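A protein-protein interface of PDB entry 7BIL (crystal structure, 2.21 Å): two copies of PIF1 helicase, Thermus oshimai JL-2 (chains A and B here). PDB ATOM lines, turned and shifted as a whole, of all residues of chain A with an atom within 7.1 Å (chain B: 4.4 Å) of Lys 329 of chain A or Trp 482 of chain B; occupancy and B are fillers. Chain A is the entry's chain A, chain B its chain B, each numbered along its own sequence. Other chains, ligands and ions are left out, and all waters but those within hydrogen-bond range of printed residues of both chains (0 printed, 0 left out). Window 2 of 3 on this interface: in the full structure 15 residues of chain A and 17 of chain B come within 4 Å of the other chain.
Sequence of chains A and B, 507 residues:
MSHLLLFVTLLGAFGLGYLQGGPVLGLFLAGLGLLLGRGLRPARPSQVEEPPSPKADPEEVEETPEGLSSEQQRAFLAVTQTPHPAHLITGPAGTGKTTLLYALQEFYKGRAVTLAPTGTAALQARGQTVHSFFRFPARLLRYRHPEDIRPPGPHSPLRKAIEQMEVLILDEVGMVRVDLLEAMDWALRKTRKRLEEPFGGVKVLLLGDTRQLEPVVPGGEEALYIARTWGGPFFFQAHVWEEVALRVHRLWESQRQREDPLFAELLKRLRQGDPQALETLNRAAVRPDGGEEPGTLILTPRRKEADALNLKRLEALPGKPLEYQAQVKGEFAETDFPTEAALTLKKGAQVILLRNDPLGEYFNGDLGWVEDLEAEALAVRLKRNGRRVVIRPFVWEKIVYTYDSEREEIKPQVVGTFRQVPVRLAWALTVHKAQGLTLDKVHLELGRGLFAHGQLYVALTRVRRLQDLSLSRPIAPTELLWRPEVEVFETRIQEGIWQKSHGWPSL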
ATOM      1  N   GLN A 327      27.716   9.655  11.194  1.00  0.00           N
ATOM      2  CA  GLN A 327      27.511  10.358  12.452  1.00  0.00           C
ATOM      3  C   GLN A 327      26.058  10.798  12.488  1.00  0.00           C
ATOM      4  O   GLN A 327      25.578  11.435  11.545  1.00  0.00           O
ATOM      5  CB  GLN A 327      28.453  11.548  12.590  1.00  0.00           C
ATOM      6  CG  GLN A 327      29.912  11.150  12.491  1.00  0.00           C
ATOM      7  CD  GLN A 327      30.808  12.326  12.180  1.00  0.00           C
ATOM      8  OE1 GLN A 327      30.464  13.477  12.470  1.00  0.00           O
ATOM      9  NE2 GLN A 327      31.965  12.047  11.580  1.00  0.00           N
ATOM     10  N   VAL A 328      25.335  10.343  13.507  1.00  0.00           N
ATOM     11  CA  VAL A 328      23.928  10.671  13.681  1.00  0.00           C
ATOM     12  C   VAL A 328      23.786  11.493  14.949  1.00  0.00           C
ATOM     13  O   VAL A 328      24.385  11.157  15.983  1.00  0.00           O
ATOM     14  CB  VAL A 328      23.065   9.402  13.737  1.00  0.00           C
ATOM     15  CG1 VAL A 328      21.598   9.752  13.581  1.00  0.00           C
ATOM     16  CG2 VAL A 328      23.506   8.427  12.642  1.00  0.00           C
ATOM     17  N   LYS A 329      23.006  12.574  14.871  1.00  0.00           N
ATOM     18  CA  LYS A 329      22.683  13.395  16.033  1.00  0.00           C
ATOM     19  C   LYS A 329      21.212  13.810  15.992  1.00  0.00           C
ATOM     20  O   LYS A 329      20.638  14.031  14.921  1.00  0.00           O
ATOM     21  CB  LYS A 329      23.625  14.615  16.155  1.00  0.00           C
ATOM     22  CG  LYS A 329      23.200  15.877  15.460  1.00  0.00           C
ATOM     23  CD  LYS A 329      24.306  16.929  15.564  1.00  0.00           C
ATOM     24  CE  LYS A 329      25.497  16.567  14.685  1.00  0.00           C
ATOM     25  NZ  LYS A 329      26.690  17.417  14.971  1.00  0.00           N
ATOM     26  N   GLY A 330      20.602  13.851  17.176  1.00  0.00           N
ATOM     27  CA  GLY A 330      19.201  14.142  17.425  1.00  0.00           C
ATOM     28  C   GLY A 330      18.301  12.992  17.016  1.00  0.00           C
ATOM     29  O   GLY A 330      18.688  11.825  17.040  1.00  0.00           O
ATOM     30  N   GLU A 331      17.115  13.342  16.523  1.00  0.00           N
ATOM     31  CA  GLU A 331      16.070  12.369  16.223  1.00  0.00           C
ATOM     32  C   GLU A 331      16.259  11.948  14.785  1.00  0.00           C
ATOM     33  O   GLU A 331      16.078  12.764  13.875  1.00  0.00           O
ATOM     34  CB  GLU A 331      14.670  12.953  16.460  1.00  0.00           C
ATOM     35  CG  GLU A 331      13.581  12.130  15.780  1.00  0.00           C
ATOM     36  CD  GLU A 331      12.177  12.664  16.029  1.00  0.00           C
ATOM     37  OE1 GLU A 331      12.006  13.473  16.964  1.00  0.00           O
ATOM     38  OE2 GLU A 331      11.242  12.271  15.295  1.00  0.00           O
ATOM     39  N   PHE A 332      16.620  10.688  14.556  1.00  0.00           N
ATOM     40  CA  PHE A 332      16.809  10.402  13.129  1.00  0.00           C
ATOM     41  C   PHE A 332      16.092   9.265  12.377  1.00  0.00           C
ATOM     42  O   PHE A 332      16.916   9.039  11.531  1.00  0.00           O
ATOM     43  CB  PHE A 332      18.307  10.500  12.619  1.00  0.00           C
ATOM     44  CG  PHE A 332      18.390  10.871  11.043  1.00  0.00           C
ATOM     45  CD1 PHE A 332      18.143  12.141  10.520  1.00  0.00           C
ATOM     46  CD2 PHE A 332      18.608   9.854  10.098  1.00  0.00           C
ATOM     47  CE1 PHE A 332      18.160  12.339   9.070  1.00  0.00           C
ATOM     48  CE2 PHE A 332      18.549  10.030   8.728  1.00  0.00           C
ATOM     49  CZ  PHE A 332      18.358  11.264   8.204  1.00  0.00           C
ATOM     50  N   VAL A 395      25.903  16.038   4.597  1.00  0.00           N
ATOM     51  CA  VAL A 395      24.984  16.071   5.728  1.00  0.00           C
ATOM     52  C   VAL A 395      23.546  16.039   5.207  1.00  0.00           C
ATOM     53  O   VAL A 395      23.214  16.734   4.247  1.00  0.00           O
ATOM     54  CB  VAL A 395      25.243  17.309   6.615  1.00  0.00           C
ATOM     55  CG1 VAL A 395      24.287  17.346   7.766  1.00  0.00           C
ATOM     56  CG2 VAL A 395      26.639  17.265   7.164  1.00  0.00           C
ATOM     57  N   LYS A 398      16.700  15.778   8.871  1.00  0.00           N
ATOM     58  CA  LYS A 398      15.399  15.152   9.094  1.00  0.00           C
ATOM     59  C   LYS A 398      14.409  16.240   9.496  1.00  0.00           C
ATOM     60  O   LYS A 398      14.623  16.949  10.487  1.00  0.00           O
ATOM     61  CB  LYS A 398      15.481  14.062  10.167  1.00  0.00           C
ATOM     62  CG  LYS A 398      14.157  13.445  10.548  1.00  0.00           C
ATOM     63  CD  LYS A 398      13.565  12.657   9.408  1.00  0.00           C
ATOM     64  CE  LYS A 398      12.062  12.505   9.573  1.00  0.00           C
ATOM     65  NZ  LYS A 398      11.515  11.574   8.541  1.00  0.00           N
ATOM     66  N   VAL A 415      14.964  18.054  13.205  1.00  0.00           N
ATOM     67  CA  VAL A 415      15.121  17.303  14.453  1.00  0.00           C
ATOM     68  C   VAL A 415      16.386  16.459  14.501  1.00  0.00           C
ATOM     69  O   VAL A 415      16.711  15.937  15.576  1.00  0.00           O
ATOM     70  CB  VAL A 415      13.892  16.427  14.771  1.00  0.00           C
ATOM     71  CG1 VAL A 415      12.662  17.301  14.983  1.00  0.00           C
ATOM     72  CG2 VAL A 415      13.679  15.343  13.692  1.00  0.00           C
ATOM     73  N   GLY A 416      17.054  16.224  13.377  1.00  0.00           N
ATOM     74  CA  GLY A 416      18.271  15.429  13.427  1.00  0.00           C
ATOM     75  C   GLY A 416      19.068  15.577  12.153  1.00  0.00           C
ATOM     76  O   GLY A 416      18.585  16.117  11.152  1.00  0.00           O
ATOM     77  N   THR A 417      20.320  15.108  12.211  1.00  0.00           N
ATOM     78  CA  THR A 417      21.214  15.093  11.061  1.00  0.00           C
ATOM     79  C   THR A 417      21.898  13.743  10.930  1.00  0.00           C
ATOM     80  O   THR A 417      22.065  13.003  11.899  1.00  0.00           O
ATOM     81  CB  THR A 417      22.322  16.162  11.138  1.00  0.00           C
ATOM     82  OG1 THR A 417      23.266  15.816  12.170  1.00  0.00           O
ATOM     83  CG2 THR A 417      21.727  17.522  11.382  1.00  0.00           C
ATOM     84  N   PHE A 418      22.333  13.458   9.709  1.00  0.00           N
ATOM     85  CA  PHE A 418      23.034  12.223   9.377  1.00  0.00           C
ATOM     86  C   PHE A 418      24.149  12.637   8.432  1.00  0.00           C
ATOM     87  O   PHE A 418      23.889  13.248   7.387  1.00  0.00           O
ATOM     88  CB  PHE A 418      22.017  11.245   8.750  1.00  0.00           C
ATOM     89  CG  PHE A 418      22.574   9.959   8.199  1.00  0.00           C
ATOM     90  CD1 PHE A 418      22.533   8.788   8.954  1.00  0.00           C
ATOM     91  CD2 PHE A 418      23.019   9.887   6.891  1.00  0.00           C
ATOM     92  CE1 PHE A 418      22.991   7.580   8.448  1.00  0.00           C
ATOM     93  CE2 PHE A 418      23.469   8.669   6.355  1.00  0.00           C
ATOM     94  CZ  PHE A 418      23.457   7.509   7.152  1.00  0.00           C
ATOM     95  N   ARG A 419      25.385  12.360   8.818  1.00  0.00           N
ATOM     96  CA  ARG A 419      26.550  12.701   8.015  1.00  0.00           C
ATOM     97  C   ARG A 419      27.162  11.414   7.506  1.00  0.00           C
ATOM     98  O   ARG A 419      27.534  10.549   8.305  1.00  0.00           O
ATOM     99  CB  ARG A 419      27.566  13.520   8.814  1.00  0.00           C
ATOM    100  CG  ARG A 419      28.743  14.038   7.983  1.00  0.00           C
ATOM    101  CD  ARG A 419      29.671  14.926   8.835  1.00  0.00           C
ATOM    102  NE  ARG A 419      30.777  15.491   8.065  1.00  0.00           N
ATOM    103  CZ  ARG A 419      31.997  14.966   7.997  1.00  0.00           C
ATOM    104  NH1 ARG A 419      32.283  13.854   8.654  1.00  0.00           N
ATOM    105  NH2 ARG A 419      32.935  15.556   7.266  1.00  0.00           N
ATOM    106  N   ARG B 211      39.268  22.928  19.328  1.00  0.00           N
ATOM    107  CA  ARG B 211      37.822  23.164  19.342  1.00  0.00           C
ATOM    108  C   ARG B 211      37.430  24.436  18.598  1.00  0.00           C
ATOM    109  O   ARG B 211      36.235  24.705  18.424  1.00  0.00           O
ATOM    110  CB  ARG B 211      37.280  23.139  20.772  1.00  0.00           C
ATOM    111  CG  ARG B 211      37.398  21.741  21.365  1.00  0.00           C
ATOM    112  CD  ARG B 211      36.424  21.530  22.496  1.00  0.00           C
ATOM    113  NE  ARG B 211      36.590  20.229  23.139  1.00  0.00           N
ATOM    114  CZ  ARG B 211      36.009  19.120  22.708  1.00  0.00           C
ATOM    115  NH1 ARG B 211      35.242  19.166  21.620  1.00  0.00           N
ATOM    116  NH2 ARG B 211      36.200  17.972  23.352  1.00  0.00           N
ATOM    117  N   LEU B 270      28.857  26.134  25.845  1.00  0.00           N
ATOM    118  CA  LEU B 270      28.694  26.055  24.400  1.00  0.00           C
ATOM    119  C   LEU B 270      29.849  25.272  23.768  1.00  0.00           C
ATOM    120  O   LEU B 270      29.648  24.550  22.790  1.00  0.00           O
ATOM    121  CB  LEU B 270      28.580  27.464  23.816  1.00  0.00           C
ATOM    122  CG  LEU B 270      27.242  28.151  24.103  1.00  0.00           C
ATOM    123  CD1 LEU B 270      27.288  29.661  23.794  1.00  0.00           C
ATOM    124  CD2 LEU B 270      26.110  27.469  23.326  1.00  0.00           C
ATOM    125  N   ARG B 271      31.045  25.366  24.347  1.00  0.00           N
ATOM    126  CA  ARG B 271      32.199  24.621  23.857  1.00  0.00           C
ATOM    127  C   ARG B 271      31.969  23.112  23.966  1.00  0.00           C
ATOM    128  O   ARG B 271      32.416  22.349  23.101  1.00  0.00           O
ATOM    129  CB  ARG B 271      33.431  25.057  24.652  1.00  0.00           C
ATOM    130  CG  ARG B 271      34.678  24.218  24.504  1.00  0.00           C
ATOM    131  CD  ARG B 271      35.791  24.799  25.396  1.00  0.00           C
ATOM    132  NE  ARG B 271      37.075  24.127  25.208  1.00  0.00           N
ATOM    133  CZ  ARG B 271      37.962  24.460  24.271  1.00  0.00           C
ATOM    134  NH1 ARG B 271      37.721  25.464  23.430  1.00  0.00           N
ATOM    135  NH2 ARG B 271      39.097  23.786  24.167  1.00  0.00           N
ATOM    136  N   GLY B 273      29.053  21.720  23.744  1.00  0.00           N
ATOM    137  CA  GLY B 273      27.835  21.392  23.023  1.00  0.00           C
ATOM    138  C   GLY B 273      26.617  21.224  23.904  1.00  0.00           C
ATOM    139  O   GLY B 273      25.877  20.248  23.777  1.00  0.00           O
ATOM    140  N   HIS B 453      33.775  22.963  11.515  1.00  0.00           N
ATOM    141  CA  HIS B 453      33.918  22.639  12.925  1.00  0.00           C
ATOM    142  C   HIS B 453      34.643  23.786  13.622  1.00  0.00           C
ATOM    143  O   HIS B 453      35.632  24.310  13.101  1.00  0.00           O
ATOM    144  CB  HIS B 453      34.691  21.327  13.063  1.00  0.00           C
ATOM    145  CG  HIS B 453      35.455  21.184  14.341  1.00  0.00           C
ATOM    146  ND1 HIS B 453      34.923  20.578  15.460  1.00  0.00           N
ATOM    147  CD2 HIS B 453      36.723  21.534  14.671  1.00  0.00           C
ATOM    148  CE1 HIS B 453      35.824  20.567  16.425  1.00  0.00           C
ATOM    149  NE2 HIS B 453      36.923  21.145  15.974  1.00  0.00           N
ATOM    150  N   THR B 478      21.206  21.018  16.103  1.00  0.00           N
ATOM    151  CA  THR B 478      21.563  20.204  14.946  1.00  0.00           C
ATOM    152  C   THR B 478      22.553  20.893  14.008  1.00  0.00           C
ATOM    153  O   THR B 478      23.114  20.222  13.134  1.00  0.00           O
ATOM    154  CB  THR B 478      20.297  19.816  14.173  1.00  0.00           C
ATOM    155  OG1 THR B 478      19.416  20.943  14.080  1.00  0.00           O
ATOM    156  CG2 THR B 478      19.578  18.675  14.878  1.00  0.00           C
ATOM    157  N   LEU B 480      25.352  22.545  15.067  1.00  0.00           N
ATOM    158  CA  LEU B 480      26.675  22.362  15.671  1.00  0.00           C
ATOM    159  C   LEU B 480      27.423  21.149  15.096  1.00  0.00           C
ATOM    160  O   LEU B 480      26.931  20.017  15.155  1.00  0.00           O
ATOM    161  CB  LEU B 480      26.523  22.215  17.188  1.00  0.00           C
ATOM    162  CG  LEU B 480      25.827  23.324  17.992  1.00  0.00           C
ATOM    163  CD1 LEU B 480      25.173  22.733  19.246  1.00  0.00           C
ATOM    164  CD2 LEU B 480      26.803  24.420  18.383  1.00  0.00           C
ATOM    165  N   LEU B 481      28.621  21.388  14.559  1.00  0.00           N
ATOM    166  CA  LEU B 481      29.486  20.359  13.983  1.00  0.00           C
ATOM    167  C   LEU B 481      30.569  19.924  14.971  1.00  0.00           C
ATOM    168  O   LEU B 481      31.108  20.751  15.716  1.00  0.00           O
ATOM    169  CB  LEU B 481      30.145  20.855  12.697  1.00  0.00           C
ATOM    170  CG  LEU B 481      29.276  21.637  11.713  1.00  0.00           C
ATOM    171  CD1 LEU B 481      29.292  23.126  12.024  1.00  0.00           C
ATOM    172  CD2 LEU B 481      29.746  21.407  10.292  1.00  0.00           C
ATOM    173  N   TRP B 482      30.866  18.618  14.993  1.00  0.00           N
ATOM    174  CA  TRP B 482      31.880  18.030  15.877  1.00  0.00           C
ATOM    175  C   TRP B 482      32.666  16.946  15.154  1.00  0.00           C
ATOM    176  O   TRP B 482      32.081  16.015  14.600  1.00  0.00           O
ATOM    177  CB  TRP B 482      31.260  17.427  17.144  1.00  0.00           C
ATOM    178  CG  TRP B 482      30.353  18.376  17.843  1.00  0.00           C
ATOM    179  CD1 TRP B 482      28.984  18.391  17.798  1.00  0.00           C
ATOM    180  CD2 TRP B 482      30.741  19.482  18.669  1.00  0.00           C
ATOM    181  NE1 TRP B 482      28.498  19.429  18.560  1.00  0.00           N
ATOM    182  CE2 TRP B 482      29.555  20.116  19.104  1.00  0.00           C
ATOM    183  CE3 TRP B 482      31.976  19.995  19.091  1.00  0.00           C
ATOM    184  CZ2 TRP B 482      29.567  21.235  19.938  1.00  0.00           C
ATOM    185  CZ3 TRP B 482      31.988  21.105  19.918  1.00  0.00           C
ATOM    186  CH2 TRP B 482      30.790  21.712  20.332  1.00  0.00           C
ATOM    187  N   ARG B 483      33.988  17.054  15.171  1.00  0.00           N
ATOM    188  CA  ARG B 483      34.834  16.077  14.504  1.00  0.00           C
ATOM    189  C   ARG B 483      35.271  15.023  15.515  1.00  0.00           C
ATOM    190  O   ARG B 483      35.843  15.383  16.553  1.00  0.00           O
ATOM    191  CB  ARG B 483      36.052  16.755  13.884  1.00  0.00           C
ATOM    192  CG  ARG B 483      35.961  16.965  12.369  1.00  0.00           C
ATOM    193  CD  ARG B 483      34.715  17.758  12.007  1.00  0.00           C
ATOM    194  NE  ARG B 483      34.573  18.004  10.567  1.00  0.00           N
ATOM    195  CZ  ARG B 483      33.549  18.662  10.012  1.00  0.00           C
ATOM    196  NH1 ARG B 483      32.567  19.140  10.772  1.00  0.00           N
ATOM    197  NH2 ARG B 483      33.506  18.850   8.695  1.00  0.00           N
ATOM    198  N   PRO B 484      34.998  13.732  15.280  1.00  0.00           N
ATOM    199  CA  PRO B 484      35.382  12.712  16.272  1.00  0.00           C
ATOM    200  C   PRO B 484      36.882  12.625  16.480  1.00  0.00           C
ATOM    201  O   PRO B 484      37.315  12.230  17.571  1.00  0.00           O
ATOM    202  CB  PRO B 484      34.804  11.408  15.690  1.00  0.00           C
ATOM    203  CG  PRO B 484      34.763  11.652  14.231  1.00  0.00           C
ATOM    204  CD  PRO B 484      34.455  13.125  14.053  1.00  0.00           C
ATOM    205  N   GLU B 487      37.728  14.829  19.329  1.00  0.00           N
ATOM    206  CA  GLU B 487      37.306  14.247  20.608  1.00  0.00           C
ATOM    207  C   GLU B 487      38.337  13.268  21.161  1.00  0.00           C
ATOM    208  O   GLU B 487      38.677  13.322  22.348  1.00  0.00           O
ATOM    209  CB  GLU B 487      35.956  13.543  20.462  1.00  0.00           C
ATOM    210  CG  GLU B 487      34.801  14.432  20.042  1.00  0.00           C
ATOM    211  CD  GLU B 487      34.592  15.639  20.962  1.00  0.00           C
ATOM    212  OE1 GLU B 487      34.030  16.656  20.470  1.00  0.00           O
ATOM    213  OE2 GLU B 487      34.983  15.568  22.162  1.00  0.00           O
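N of Lys 398 of chain A lies within hydrogen-bond range of O of Gly 416 of chain A, at 3.0 Å. The backbone NH (N) of Val 415 of chain A is in hydrogen-bond range of the backbone carbonyl oxygen (O) of Lys 398 of chain A (3.0 Å). N of Glu 331 of chain A is in hydrogen-bond range of O of Val 415 of chain A, 2.8 Å away. The backbone NH (N) of Thr 417 of chain A is in hydrogen-bond range of the backbone carbonyl oxygen (O) of Lys 329 of chain A (2.9 Å). N of Arg 419 of chain A lies within hydrogen-bond range of O of Gln 327 of chain A (2.9 Å).
Of the 12 printed residues of chain B, 5 touch a printed residue of chain A. Printed residues of chain B that touch a printed residue of chain A: Thr 478, Leu 480, Trp 482, Arg 483 and Pro 484. Of the 13 printed residues of chain A, 6 touch a printed residue of chain B.
Lys 329 of chain A touches just these residues of chain B: Leu 480 and Trp 482. Trp 482 of chain B touches just these residues of chain A: Gln 327 (3.7 Å) and Lys 329 (3.8 Å). Printed residues of chain A within 4 Å of Pro 484 of chain B: Gln 327 (3.7 Å). Of the printed residues of chain A, Leu 480 of chain B touches Lys 329 (2.6 Å). Printed residues of chain A within 4 Å of Thr 478 of chain B: Val 415, Gly 416 and Thr 417. Gly 273 of chain B touches none of the printed residues of chain A. Phe 332 of chain A touches none of the printed residues of chain B. The nearest residue of chain A that does not touch Trp 482 of chain B is Arg 419 of chain A (6.3 Å).
Gln 327 of chain A touches Trp 482 of chain B (OE1 to O, 3.7 Å). NE2 of Gln 327 of chain A touches CD of Pro 484 of chain B (3.7 Å). NZ of Lys 329 of chain A touches CD1 of Trp 482 of chain B, 3.8 Å away. C of Val 415 of chain A touches CG2 of Thr 478 of chain B, at 3.9 Å. CA of Gly 416 of chain A touches CG2 of Thr 478 of chain B, 3.8 Å away. Thr 478 of chain B touches Thr 417 of chain A (O to CG2, 3.5 Å). Arg 483 of chain B touches Arg 419 of chain A (NH2 to NH2, 3.6 Å).
The side-chain amino group (NZ) of Lys 329 of chain A sits at hydrogen-bond distance from the backbone carbonyl oxygen (O) of Leu 480 of chain B (2.6 Å).
No position is printed for both chains.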
